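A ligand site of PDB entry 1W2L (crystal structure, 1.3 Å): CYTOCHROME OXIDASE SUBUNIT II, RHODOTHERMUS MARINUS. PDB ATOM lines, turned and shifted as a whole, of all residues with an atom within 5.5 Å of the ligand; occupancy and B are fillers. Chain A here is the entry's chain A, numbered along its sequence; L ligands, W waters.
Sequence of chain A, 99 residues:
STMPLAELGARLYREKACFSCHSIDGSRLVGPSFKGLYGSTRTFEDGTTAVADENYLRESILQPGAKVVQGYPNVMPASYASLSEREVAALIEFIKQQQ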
ATOM      1  N   LEU A  12     -34.839 -10.325  24.365  1.00  0.00           N
ATOM      2  CA  LEU A  12     -33.541  -9.746  24.041  1.00  0.00           C
ATOM      3  C   LEU A  12     -32.424 -10.769  24.298  1.00  0.00           C
ATOM      4  O   LEU A  12     -31.443 -10.733  23.560  1.00  0.00           O
ATOM      5  CB  LEU A  12     -33.298  -8.500  24.865  1.00  0.00           C
ATOM      6  CG  LEU A  12     -34.203  -7.290  24.531  1.00  0.00           C
ATOM      7  CD1 LEU A  12     -34.069  -6.253  25.619  1.00  0.00           C
ATOM      8  CD2 LEU A  12     -33.875  -6.730  23.167  1.00  0.00           C
ATOM      9  N   LYS A  16     -30.517 -10.573  20.882  1.00  0.00           N
ATOM     10  CA  LYS A  16     -29.245  -9.900  20.972  1.00  0.00           C
ATOM     11  C   LYS A  16     -28.052 -10.876  21.128  1.00  0.00           C
ATOM     12  O   LYS A  16     -26.954 -10.427  21.331  1.00  0.00           O
ATOM     13  CB  LYS A  16     -29.240  -8.861  22.099  1.00  0.00           C
ATOM     14  CG  LYS A  16     -30.319  -7.803  21.932  1.00  0.00           C
ATOM     15  CD  LYS A  16     -29.934  -6.901  20.764  1.00  0.00           C
ATOM     16  CE  LYS A  16     -30.852  -5.711  20.653  1.00  0.00           C
ATOM     17  NZ  LYS A  16     -30.549  -4.928  19.417  1.00  0.00           N
ATOM     18  N   ALA A  17     -28.312 -12.152  21.013  1.00  0.00           N
ATOM     19  CA  ALA A  17     -27.294 -13.205  20.915  1.00  0.00           C
ATOM     20  C   ALA A  17     -26.686 -13.620  22.249  1.00  0.00           C
ATOM     21  O   ALA A  17     -25.764 -14.408  22.233  1.00  0.00           O
ATOM     22  CB  ALA A  17     -26.211 -12.816  19.907  1.00  0.00           C
ATOM     23  N   CYS A  18     -27.204 -13.117  23.366  1.00  0.00           N
ATOM     24  CA  CYS A  18     -26.612 -13.476  24.661  1.00  0.00           C
ATOM     25  C   CYS A  18     -26.580 -14.996  24.863  1.00  0.00           C
ATOM     26  O   CYS A  18     -25.647 -15.520  25.414  1.00  0.00           O
ATOM     27  CB  CYS A  18     -27.401 -12.839  25.808  1.00  0.00           C
ATOM     28  SG  CYS A  18     -27.915 -11.135  25.593  1.00  0.00           S
ATOM     29  N   SER A  20     -25.907 -17.290  23.031  1.00  0.00           N
ATOM     30  CA  SER A  20     -24.851 -17.992  22.342  1.00  0.00           C
ATOM     31  C   SER A  20     -23.626 -18.185  23.250  1.00  0.00           C
ATOM     32  O   SER A  20     -22.806 -19.094  23.034  1.00  0.00           O
ATOM     33  CB  SER A  20     -24.458 -17.325  21.039  1.00  0.00           C
ATOM     34  OG  SER A  20     -23.887 -16.050  21.175  1.00  0.00           O
ATOM     35  N   CYS A  21     -23.477 -17.337  24.239  1.00  0.00           N
ATOM     36  CA  CYS A  21     -22.332 -17.377  25.142  1.00  0.00           C
ATOM     37  C   CYS A  21     -22.717 -17.577  26.602  1.00  0.00           C
ATOM     38  O   CYS A  21     -21.831 -17.861  27.397  1.00  0.00           O
ATOM     39  CB  CYS A  21     -21.496 -16.090  25.009  1.00  0.00           C
ATOM     40  SG  CYS A  21     -20.765 -15.939  23.361  1.00  0.00           S
ATOM     41  N   HIS A  22     -24.001 -17.386  26.940  1.00  0.00           N
ATOM     42  CA  HIS A  22     -24.430 -17.453  28.351  1.00  0.00           C
ATOM     43  C   HIS A  22     -25.658 -18.336  28.467  1.00  0.00           C
ATOM     44  O   HIS A  22     -26.714 -18.017  27.878  1.00  0.00           O
ATOM     45  CB  HIS A  22     -24.854 -16.045  28.812  1.00  0.00           C
ATOM     46  CG  HIS A  22     -23.747 -15.041  28.920  1.00  0.00           C
ATOM     47  ND1 HIS A  22     -22.778 -15.078  29.899  1.00  0.00           N
ATOM     48  CD2 HIS A  22     -23.493 -13.940  28.163  1.00  0.00           C
ATOM     49  CE1 HIS A  22     -21.964 -14.019  29.725  1.00  0.00           C
ATOM     50  NE2 HIS A  22     -22.397 -13.337  28.676  1.00  0.00           N
ATOM     51  N   VAL A  30     -19.050 -20.190  26.271  1.00  0.00           N
ATOM     52  CA  VAL A  30     -17.946 -19.256  26.148  1.00  0.00           C
ATOM     53  C   VAL A  30     -17.873 -18.366  27.379  1.00  0.00           C
ATOM     54  O   VAL A  30     -16.807 -18.082  27.892  1.00  0.00           O
ATOM     55  CB  VAL A  30     -18.086 -18.500  24.831  1.00  0.00           C
ATOM     56  CG1 VAL A  30     -17.164 -17.316  24.761  1.00  0.00           C
ATOM     57  CG2 VAL A  30     -17.767 -19.417  23.645  1.00  0.00           C
ATOM     58  N   GLY A  31     -19.007 -17.882  27.823  1.00  0.00           N
ATOM     59  CA  GLY A  31     -19.117 -17.067  29.013  1.00  0.00           C
ATOM     60  C   GLY A  31     -19.801 -17.827  30.168  1.00  0.00           C
ATOM     61  O   GLY A  31     -20.245 -18.971  30.025  1.00  0.00           O
ATOM     62  N   PRO A  32     -19.819 -17.173  31.305  1.00  0.00           N
ATOM     63  CA  PRO A  32     -20.434 -17.754  32.520  1.00  0.00           C
ATOM     64  C   PRO A  32     -21.936 -17.827  32.417  1.00  0.00           C
ATOM     65  O   PRO A  32     -22.611 -17.033  31.777  1.00  0.00           O
ATOM     66  CB  PRO A  32     -19.985 -16.832  33.621  1.00  0.00           C
ATOM     67  CG  PRO A  32     -19.691 -15.535  32.924  1.00  0.00           C
ATOM     68  CD  PRO A  32     -19.196 -15.875  31.556  1.00  0.00           C
ATOM     69  N   SER A  33     -22.501 -18.804  33.151  1.00  0.00           N
ATOM     70  CA  SER A  33     -23.947 -18.890  33.156  1.00  0.00           C
ATOM     71  C   SER A  33     -24.562 -17.718  33.891  1.00  0.00           C
ATOM     72  O   SER A  33     -24.012 -17.184  34.856  1.00  0.00           O
ATOM     73  CB  SER A  33     -24.353 -20.196  33.853  1.00  0.00           C
ATOM     74  OG  SER A  33     -25.733 -20.448  33.704  1.00  0.00           O
ATOM     75  N   PHE A  34     -25.770 -17.331  33.464  1.00  0.00           N
ATOM     76  CA  PHE A  34     -26.563 -16.339  34.193  1.00  0.00           C
ATOM     77  C   PHE A  34     -27.292 -16.899  35.394  1.00  0.00           C
ATOM     78  O   PHE A  34     -27.727 -16.172  36.257  1.00  0.00           O
ATOM     79  CB  PHE A  34     -27.605 -15.728  33.276  1.00  0.00           C
ATOM     80  CG  PHE A  34     -27.088 -14.790  32.212  1.00  0.00           C
ATOM     81  CD1 PHE A  34     -25.834 -14.191  32.285  1.00  0.00           C
ATOM     82  CD2 PHE A  34     -27.871 -14.509  31.131  1.00  0.00           C
ATOM     83  CE1 PHE A  34     -25.445 -13.286  31.317  1.00  0.00           C
ATOM     84  CE2 PHE A  34     -27.471 -13.586  30.173  1.00  0.00           C
ATOM     85  CZ  PHE A  34     -26.245 -12.999  30.253  1.00  0.00           C
ATOM     86  N   LEU A  37     -26.309 -15.649  38.933  1.00  0.00           N
ATOM     87  CA  LEU A  37     -25.359 -14.573  38.785  1.00  0.00           C
ATOM     88  C   LEU A  37     -25.666 -13.385  39.692  1.00  0.00           C
ATOM     89  O   LEU A  37     -24.838 -12.890  40.440  1.00  0.00           O
ATOM     90  CB  LEU A  37     -25.302 -14.121  37.316  1.00  0.00           C
ATOM     91  CG  LEU A  37     -24.572 -12.832  37.036  1.00  0.00           C
ATOM     92  CD1 LEU A  37     -23.133 -12.865  37.575  1.00  0.00           C
ATOM     93  CD2 LEU A  37     -24.569 -12.520  35.541  1.00  0.00           C
ATOM     94  N   ARG A  42     -18.075 -12.026  42.292  1.00  0.00           N
ATOM     95  CA  ARG A  42     -17.246 -12.205  41.122  1.00  0.00           C
ATOM     96  C   ARG A  42     -15.788 -11.903  41.434  1.00  0.00           C
ATOM     97  O   ARG A  42     -15.501 -10.933  42.126  1.00  0.00           O
ATOM     98  CB  ARG A  42     -17.714 -11.333  39.966  1.00  0.00           C
ATOM     99  CG  ARG A  42     -19.186 -11.235  39.732  1.00  0.00           C
ATOM    100  CD  ARG A  42     -19.939 -12.529  39.680  1.00  0.00           C
ATOM    101  NE  ARG A  42     -19.553 -13.395  38.599  1.00  0.00           N
ATOM    102  CZ  ARG A  42     -19.141 -14.638  38.602  1.00  0.00           C
ATOM    103  NH1 ARG A  42     -18.873 -15.230  37.441  1.00  0.00           N
ATOM    104  NH2 ARG A  42     -18.976 -15.317  39.744  1.00  0.00           N
ATOM    105  N   ALA A  52     -22.137  -8.993  42.198  1.00  0.00           N
ATOM    106  CA  ALA A  52     -22.923  -8.777  41.002  1.00  0.00           C
ATOM    107  C   ALA A  52     -24.264  -8.139  41.323  1.00  0.00           C
ATOM    108  O   ALA A  52     -25.315  -8.781  41.360  1.00  0.00           O
ATOM    109  CB  ALA A  52     -23.082 -10.070  40.198  1.00  0.00           C
ATOM    110  N   TYR A  56     -23.132  -3.555  38.508  1.00  0.00           N
ATOM    111  CA  TYR A  56     -22.186  -4.445  37.865  1.00  0.00           C
ATOM    112  C   TYR A  56     -22.744  -5.045  36.585  1.00  0.00           C
ATOM    113  O   TYR A  56     -22.028  -5.169  35.585  1.00  0.00           O
ATOM    114  CB  TYR A  56     -21.747  -5.563  38.842  1.00  0.00           C
ATOM    115  CG  TYR A  56     -20.993  -6.660  38.130  1.00  0.00           C
ATOM    116  CD1 TYR A  56     -19.682  -6.431  37.735  1.00  0.00           C
ATOM    117  CD2 TYR A  56     -21.557  -7.845  37.784  1.00  0.00           C
ATOM    118  CE1 TYR A  56     -18.967  -7.385  37.057  1.00  0.00           C
ATOM    119  CE2 TYR A  56     -20.843  -8.812  37.104  1.00  0.00           C
ATOM    120  CZ  TYR A  56     -19.540  -8.585  36.733  1.00  0.00           C
ATOM    121  OH  TYR A  56     -18.806  -9.513  36.064  1.00  0.00           O
ATOM    122  N   LEU A  57     -23.999  -5.455  36.606  1.00  0.00           N
ATOM    123  CA  LEU A  57     -24.595  -6.012  35.408  1.00  0.00           C
ATOM    124  C   LEU A  57     -24.655  -4.955  34.305  1.00  0.00           C
ATOM    125  O   LEU A  57     -24.354  -5.229  33.154  1.00  0.00           O
ATOM    126  CB  LEU A  57     -25.972  -6.581  35.716  1.00  0.00           C
ATOM    127  CG  LEU A  57     -26.002  -7.742  36.702  1.00  0.00           C
ATOM    128  CD1 LEU A  57     -27.451  -8.190  36.966  1.00  0.00           C
ATOM    129  CD2 LEU A  57     -25.167  -8.890  36.210  1.00  0.00           C
ATOM    130  N   SER A  60     -21.191  -4.365  32.931  1.00  0.00           N
ATOM    131  CA  SER A  60     -20.780  -5.510  32.157  1.00  0.00           C
ATOM    132  C   SER A  60     -21.354  -5.474  30.730  1.00  0.00           C
ATOM    133  O   SER A  60     -20.649  -5.883  29.783  1.00  0.00           O
ATOM    134  CB  SER A  60     -21.208  -6.806  32.852  1.00  0.00           C
ATOM    135  OG  SER A  60     -20.518  -7.019  34.046  1.00  0.00           O
ATOM    136  N   ILE A  61     -22.553  -4.980  30.593  1.00  0.00           N
ATOM    137  CA  ILE A  61     -23.245  -4.935  29.309  1.00  0.00           C
ATOM    138  C   ILE A  61     -22.833  -3.718  28.512  1.00  0.00           C
ATOM    139  O   ILE A  61     -22.543  -3.805  27.309  1.00  0.00           O
ATOM    140  CB  ILE A  61     -24.779  -4.983  29.547  1.00  0.00           C
ATOM    141  CG1 ILE A  61     -25.191  -6.308  30.180  1.00  0.00           C
ATOM    142  CG2 ILE A  61     -25.528  -4.736  28.250  1.00  0.00           C
ATOM    143  CD1 ILE A  61     -26.604  -6.330  30.724  1.00  0.00           C
ATOM    144  N   GLY A  65     -15.715  -5.493  28.425  1.00  0.00           N
ATOM    145  CA  GLY A  65     -14.273  -5.571  28.417  1.00  0.00           C
ATOM    146  C   GLY A  65     -13.698  -4.715  29.532  1.00  0.00           C
ATOM    147  O   GLY A  65     -12.514  -4.896  29.766  1.00  0.00           O
ATOM    148  N   LYS A  67     -14.190  -4.775  33.089  1.00  0.00           N
ATOM    149  CA  LYS A  67     -13.738  -5.658  34.174  1.00  0.00           C
ATOM    150  C   LYS A  67     -14.039  -7.082  33.678  1.00  0.00           C
ATOM    151  O   LYS A  67     -15.204  -7.299  33.237  1.00  0.00           O
ATOM    152  CB  LYS A  67     -14.391  -5.507  35.529  1.00  0.00           C
ATOM    153  CG  LYS A  67     -13.951  -4.345  36.385  1.00  0.00           C
ATOM    154  CD  LYS A  67     -14.635  -4.342  37.747  1.00  0.00           C
ATOM    155  CE  LYS A  67     -14.689  -2.956  38.398  1.00  0.00           C
ATOM    156  NZ  LYS A  67     -14.906  -2.976  39.878  1.00  0.00           N
ATOM    157  N   VAL A  68     -13.117  -7.973  33.687  1.00  0.00           N
ATOM    158  CA  VAL A  68     -13.287  -9.306  33.092  1.00  0.00           C
ATOM    159  C   VAL A  68     -13.203 -10.401  34.139  1.00  0.00           C
ATOM    160  O   VAL A  68     -12.206 -10.489  34.868  1.00  0.00           O
ATOM    161  CB  VAL A  68     -12.206  -9.540  32.026  1.00  0.00           C
ATOM    162  CG1 VAL A  68     -12.348 -10.892  31.335  1.00  0.00           C
ATOM    163  CG2 VAL A  68     -12.222  -8.411  30.996  1.00  0.00           C
ATOM    164  N   VAL A  69     -14.220 -11.265  34.194  1.00  0.00           N
ATOM    165  CA  VAL A  69     -14.228 -12.395  35.147  1.00  0.00           C
ATOM    166  C   VAL A  69     -13.016 -13.282  34.921  1.00  0.00           C
ATOM    167  O   VAL A  69     -12.680 -13.655  33.785  1.00  0.00           O
ATOM    168  CB  VAL A  69     -15.563 -13.157  35.019  1.00  0.00           C
ATOM    169  CG1 VAL A  69     -15.602 -14.371  35.915  1.00  0.00           C
ATOM    170  CG2 VAL A  69     -16.742 -12.243  35.272  1.00  0.00           C
ATOM    171  N   TYR A  72     -11.990 -16.436  31.997  1.00  0.00           N
ATOM    172  CA  TYR A  72     -12.763 -16.288  30.765  1.00  0.00           C
ATOM    173  C   TYR A  72     -12.034 -15.445  29.758  1.00  0.00           C
ATOM    174  O   TYR A  72     -11.324 -14.506  30.104  1.00  0.00           O
ATOM    175  CB  TYR A  72     -14.147 -15.681  31.073  1.00  0.00           C
ATOM    176  CG  TYR A  72     -15.073 -16.639  31.741  1.00  0.00           C
ATOM    177  CD1 TYR A  72     -15.800 -17.520  30.954  1.00  0.00           C
ATOM    178  CD2 TYR A  72     -15.230 -16.688  33.114  1.00  0.00           C
ATOM    179  CE1 TYR A  72     -16.647 -18.398  31.548  1.00  0.00           C
ATOM    180  CE2 TYR A  72     -16.085 -17.602  33.714  1.00  0.00           C
ATOM    181  CZ  TYR A  72     -16.812 -18.473  32.898  1.00  0.00           C
ATOM    182  OH  TYR A  72     -17.686 -19.405  33.374  1.00  0.00           O
ATOM    183  N   PRO A  73     -12.282 -15.683  28.463  1.00  0.00           N
ATOM    184  CA  PRO A  73     -11.720 -14.805  27.438  1.00  0.00           C
ATOM    185  C   PRO A  73     -12.456 -13.476  27.378  1.00  0.00           C
ATOM    186  O   PRO A  73     -13.645 -13.404  27.668  1.00  0.00           O
ATOM    187  CB  PRO A  73     -11.963 -15.618  26.144  1.00  0.00           C
ATOM    188  CG  PRO A  73     -13.224 -16.384  26.437  1.00  0.00           C
ATOM    189  CD  PRO A  73     -13.121 -16.742  27.924  1.00  0.00           C
ATOM    190  N   ASN A  74     -11.753 -12.431  26.951  1.00  0.00           N
ATOM    191  CA  ASN A  74     -12.302 -11.086  26.890  1.00  0.00           C
ATOM    192  C   ASN A  74     -12.949 -10.830  25.541  1.00  0.00           C
ATOM    193  O   ASN A  74     -12.382 -10.217  24.684  1.00  0.00           O
ATOM    194  CB  ASN A  74     -11.188 -10.101  27.258  1.00  0.00           C
ATOM    195  CG  ASN A  74     -11.690  -8.661  27.420  1.00  0.00           C
ATOM    196  OD1 ASN A  74     -12.878  -8.427  27.280  1.00  0.00           O
ATOM    197  ND2 ASN A  74     -10.800  -7.735  27.656  1.00  0.00           N
ATOM    198  N   VAL A  75     -14.142 -11.394  25.370  1.00  0.00           N
ATOM    199  CA  VAL A  75     -14.817 -11.401  24.084  1.00  0.00           C
ATOM    200  C   VAL A  75     -16.224 -10.830  24.139  1.00  0.00           C
ATOM    201  O   VAL A  75     -16.936 -10.935  23.155  1.00  0.00           O
ATOM    202  CB  VAL A  75     -14.822 -12.809  23.437  1.00  0.00           C
ATOM    203  CG1 VAL A  75     -13.403 -13.232  23.105  1.00  0.00           C
ATOM    204  CG2 VAL A  75     -15.546 -13.827  24.287  1.00  0.00           C
ATOM    205  N   MET A  76     -16.644 -10.129  25.194  1.00  0.00           N
ATOM    206  CA  MET A  76     -17.962  -9.499  25.211  1.00  0.00           C
ATOM    207  C   MET A  76     -18.091  -8.546  24.028  1.00  0.00           C
ATOM    208  O   MET A  76     -17.230  -7.665  23.854  1.00  0.00           O
ATOM    209  CB  MET A  76     -18.203  -8.737  26.538  1.00  0.00           C
ATOM    210  CG  MET A  76     -18.920  -9.485  27.631  1.00  0.00           C
ATOM    211  SD  MET A  76     -20.671  -9.653  27.302  1.00  0.00           S
ATOM    212  CE  MET A  76     -21.445  -8.261  27.910  1.00  0.00           C
ATOM    213  N   PRO A  77     -19.156  -8.623  23.240  1.00  0.00           N
ATOM    214  CA  PRO A  77     -19.354  -7.738  22.089  1.00  0.00           C
ATOM    215  C   PRO A  77     -19.397  -6.264  22.380  1.00  0.00           C
ATOM    216  O   PRO A  77     -19.977  -5.813  23.338  1.00  0.00           O
ATOM    217  CB  PRO A  77     -20.716  -8.183  21.523  1.00  0.00           C
ATOM    218  CG  PRO A  77     -20.745  -9.641  21.848  1.00  0.00           C
ATOM    219  CD  PRO A  77     -20.108  -9.746  23.202  1.00  0.00           C
ATOM    220  N   TYR A  80     -23.163  -3.980  22.330  1.00  0.00           N
ATOM    221  CA  TYR A  80     -24.114  -3.754  23.407  1.00  0.00           C
ATOM    222  C   TYR A  80     -23.960  -2.366  24.037  1.00  0.00           C
ATOM    223  O   TYR A  80     -24.860  -1.954  24.790  1.00  0.00           O
ATOM    224  CB  TYR A  80     -23.980  -4.843  24.471  1.00  0.00           C
ATOM    225  CG  TYR A  80     -24.171  -6.215  23.865  1.00  0.00           C
ATOM    226  CD1 TYR A  80     -25.083  -6.506  22.880  1.00  0.00           C
ATOM    227  CD2 TYR A  80     -23.357  -7.260  24.274  1.00  0.00           C
ATOM    228  CE1 TYR A  80     -25.205  -7.758  22.347  1.00  0.00           C
ATOM    229  CE2 TYR A  80     -23.476  -8.509  23.772  1.00  0.00           C
ATOM    230  CZ  TYR A  80     -24.401  -8.799  22.791  1.00  0.00           C
ATOM    231  OH  TYR A  80     -24.503 -10.067  22.302  1.00  0.00           O
ATOM    232  N   LEU A  83     -27.074  -0.391  23.484  1.00  0.00           N
ATOM    233  CA  LEU A  83     -28.409  -0.728  23.965  1.00  0.00           C
ATOM    234  C   LEU A  83     -29.067   0.444  24.681  1.00  0.00           C
ATOM    235  O   LEU A  83     -28.424   1.197  25.420  1.00  0.00           O
ATOM    236  CB  LEU A  83     -28.339  -1.937  24.902  1.00  0.00           C
ATOM    237  CG  LEU A  83     -27.949  -3.262  24.264  1.00  0.00           C
ATOM    238  CD1 LEU A  83     -27.597  -4.261  25.340  1.00  0.00           C
ATOM    239  CD2 LEU A  83     -29.042  -3.777  23.341  1.00  0.00           C
ATOM    240  N   LEU A  91     -32.934  -6.665  30.146  1.00  0.00           N
ATOM    241  CA  LEU A  91     -31.962  -7.733  30.260  1.00  0.00           C
ATOM    242  C   LEU A  91     -31.633  -8.003  31.714  1.00  0.00           C
ATOM    243  O   LEU A  91     -31.479  -9.129  32.142  1.00  0.00           O
ATOM    244  CB  LEU A  91     -30.686  -7.415  29.478  1.00  0.00           C
ATOM    245  CG  LEU A  91     -30.822  -7.594  27.957  1.00  0.00           C
ATOM    246  CD1 LEU A  91     -29.748  -6.818  27.236  1.00  0.00           C
ATOM    247  CD2 LEU A  91     -30.786  -9.042  27.523  1.00  0.00           C
ATOM    248  N   ILE A  95     -32.019 -11.375  33.871  1.00  0.00           N
ATOM    249  CA  ILE A  95     -30.895 -12.007  34.602  1.00  0.00           C
ATOM    250  C   ILE A  95     -31.219 -12.200  36.065  1.00  0.00           C
ATOM    251  O   ILE A  95     -30.899 -13.284  36.587  1.00  0.00           O
ATOM    252  CB  ILE A  95     -29.576 -11.221  34.441  1.00  0.00           C
ATOM    253  CG1 ILE A  95     -29.116 -11.240  33.008  1.00  0.00           C
ATOM    254  CG2 ILE A  95     -28.506 -11.699  35.414  1.00  0.00           C
ATOM    255  CD1 ILE A  95     -27.978 -10.279  32.751  1.00  0.00           C
HETATM  256 FE1  LIG L   1     -21.571 -11.584  28.103  1.00  0.00          FE
HETATM  257  C1  LIG L   1     -19.578 -11.611  30.886  1.00  0.00           C
HETATM  258  C2  LIG L   1     -24.027 -10.042  29.892  1.00  0.00           C
HETATM  259  C3  LIG L   1     -23.501 -11.477  25.313  1.00  0.00           C
HETATM  260  C4  LIG L   1     -19.251 -13.455  26.429  1.00  0.00           C
HETATM  261  N1  LIG L   1     -21.746 -10.940  30.015  1.00  0.00           N
HETATM  262  C5  LIG L   1     -20.790 -11.021  31.012  1.00  0.00           C
HETATM  263  C6  LIG L   1     -21.400 -10.578  32.231  1.00  0.00           C
HETATM  264  C7  LIG L   1     -22.614 -10.093  31.949  1.00  0.00           C
HETATM  265  C8  LIG L   1     -22.870 -10.315  30.532  1.00  0.00           C
HETATM  266  C9  LIG L   1     -23.680  -9.545  32.902  1.00  0.00           C
HETATM  267  C10 LIG L   1     -20.741 -10.752  33.600  1.00  0.00           C
HETATM  268  C11 LIG L   1     -21.030 -12.200  34.016  1.00  0.00           C
HETATM  269  C12 LIG L   1     -20.438 -12.683  35.387  1.00  0.00           C
HETATM  270  O1  LIG L   1     -20.495 -13.883  35.518  1.00  0.00           O
HETATM  271  O2  LIG L   1     -19.921 -11.825  36.149  1.00  0.00           O
HETATM  272  N2  LIG L   1     -23.423 -10.897  27.688  1.00  0.00           N
HETATM  273  C13 LIG L   1     -24.245 -10.352  28.566  1.00  0.00           C
HETATM  274  C14 LIG L   1     -25.534 -10.006  27.914  1.00  0.00           C
HETATM  275  C15 LIG L   1     -25.344 -10.354  26.595  1.00  0.00           C
HETATM  276  C16 LIG L   1     -24.054 -10.944  26.456  1.00  0.00           C
HETATM  277  C17 LIG L   1     -26.725  -9.458  28.587  1.00  0.00           C
HETATM  278  C18 LIG L   1     -26.305 -10.188  25.444  1.00  0.00           C
HETATM  279  C19 LIG L   1     -26.751  -8.713  25.330  1.00  0.00           C
HETATM  280  N3  LIG L   1     -21.411 -12.262  26.242  1.00  0.00           N
HETATM  281  C20 LIG L   1     -22.346 -12.116  25.229  1.00  0.00           C
HETATM  282  C21 LIG L   1     -21.822 -12.826  24.035  1.00  0.00           C
HETATM  283  C22 LIG L   1     -20.651 -13.360  24.354  1.00  0.00           C
HETATM  284  C23 LIG L   1     -20.352 -13.014  25.714  1.00  0.00           C
HETATM  285  C24 LIG L   1     -22.620 -12.894  22.723  1.00  0.00           C
HETATM  286  C25 LIG L   1     -19.800 -14.341  23.546  1.00  0.00           C
HETATM  287  C26 LIG L   1     -19.289 -13.881  22.194  1.00  0.00           C
HETATM  288  N4  LIG L   1     -19.762 -12.336  28.562  1.00  0.00           N
HETATM  289  C27 LIG L   1     -18.988 -13.106  27.748  1.00  0.00           C
HETATM  290  C28 LIG L   1     -17.799 -13.556  28.455  1.00  0.00           C
HETATM  291  C29 LIG L   1     -17.913 -13.009  29.667  1.00  0.00           C
HETATM  292  C30 LIG L   1     -19.099 -12.253  29.769  1.00  0.00           C
HETATM  293  C31 LIG L   1     -16.770 -14.436  27.884  1.00  0.00           C
HETATM  294  C32 LIG L   1     -16.883 -13.186  30.848  1.00  0.00           C
HETATM  295  C33 LIG L   1     -15.699 -12.224  30.715  1.00  0.00           C
HETATM  296  C34 LIG L   1     -16.079 -10.844  31.137  1.00  0.00           C
HETATM  297  O3  LIG L   1     -16.142  -9.904  30.281  1.00  0.00           O
HETATM  298  O4  LIG L   1     -16.373 -10.643  32.348  1.00  0.00           O
HETATM  299  O   HOH W   1     -16.274  -7.377  30.483  1.00  0.00           O
HETATM  300  O   HOH W   2     -17.750  -8.498  33.419  1.00  0.00           O
HETATM  301  O   HOH W   3     -18.831  -7.816  30.790  1.00  0.00           O
HETATM  302  O   HOH W   4     -15.347  -9.740  27.728  1.00  0.00           O
HETATM  303  O   HOH W   5     -22.065 -16.162  36.414  1.00  0.00           O
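Merely in contact with the ligand: Pro 32 (3.2 Å), Pro 73 (3.3 Å), Tyr 80 (3.3 Å), Val 68 (3.4 Å), Leu 37 (3.5 Å), Ala 17 (3.5 Å), Pro 77 (3.6 Å), Val 30 (3.6 Å), Lys 67 (3.7 Å), Leu 57 (3.7 Å), Ser 60 (3.7 Å), Gly 31 (3.7 Å), Tyr 72 (3.7 Å), Phe 34 (3.7 Å), Ser 20 (3.7 Å), Ile 61 (3.8 Å) and Val 75 (3.8 Å). Hydrophobic or aromatic side chains that line the ligand: His 22, Pro 32, Phe 34, Leu 37, Tyr 56, Leu 57, Ile 61, Val 68, Val 69, Tyr 72, Val 75, Met 76, Pro 77 and Tyr 80. The nearest printed residue that does not touch the ligand is Leu 91 (4.03 Å).
Water W1 lies within hydrogen-bond range of an oxygen (O3) of the ligand (2.5 Å), the backbone NH (N) of Gly 65 (2.8 Å) and the backbone carbonyl oxygen (O) of Lys 67 (3.0 Å). Water W4 lies within hydrogen-bond range of O3 of the ligand (2.7 Å), OD1 of Asn 74 (2.8 Å), N of Met 76 (2.9 Å) and N of Val 75 (3.1 Å). Water W2 lies within hydrogen-bond range of O4 of the ligand (2.8 Å), O of Lys 67 (2.8 Å), OH of Tyr 56 (3.0 Å) and OG of Ser 60 (3.2 Å). Water W5 lies within hydrogen-bond range of the backbone carbonyl oxygen of Ser 33, an oxygen (O1) of the ligand and the guanidinium group of Arg 42. Water W3 bridges the backbone carbonyl oxygen of Ser 60 (2.8 Å) and an oxygen (O3) of the ligand (3.4 Å).
The side-chain sulfur of Cys 18 is covalently linked to a carbon (C18) of the ligand (1.9 Å). A carbon (C25) of the ligand is bonded to the side-chain sulfur of Cys 21 (1.9 Å). An iron atom (FE1) of the ligand is bound by a ring nitrogen (NE2) of His 22 (2.0 Å). The side-chain sulfur (SD) of Met 76 is bound to an iron atom (FE1) of the ligand (2.3 Å). The side-chain hydroxyl of Tyr 56 lies within hydrogen-bond range of an oxygen (O2) of the ligand, 2.6 Å away. O1 of the ligand is in salt-bridge range of NH1 of Arg 42 (2.9 Å). O4 of the ligand sits at hydrogen-bond distance from N of Val 69, 2.9 Å away.
The backbone NH (N) of Gly 31 sits at hydrogen-bond distance from the backbone carbonyl oxygen (O) of Cys 21, 2.9 Å away. A ring nitrogen (ND1) of His 22 is in hydrogen-bond range of the backbone carbonyl oxygen (O) of Pro 32, at 2.7 Å. The backbone carbonyl oxygen of Tyr 56 lies within hydrogen-bond range of the side-chain hydroxyl of Ser 60. The backbone carbonyl oxygen (O) of Lys 16 is in hydrogen-bond range of the side-chain hydroxyl (OH) of Tyr 80 (2.7 Å). O of Ala 17 sits at hydrogen-bond distance from OG of Ser 20 (2.7 Å).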
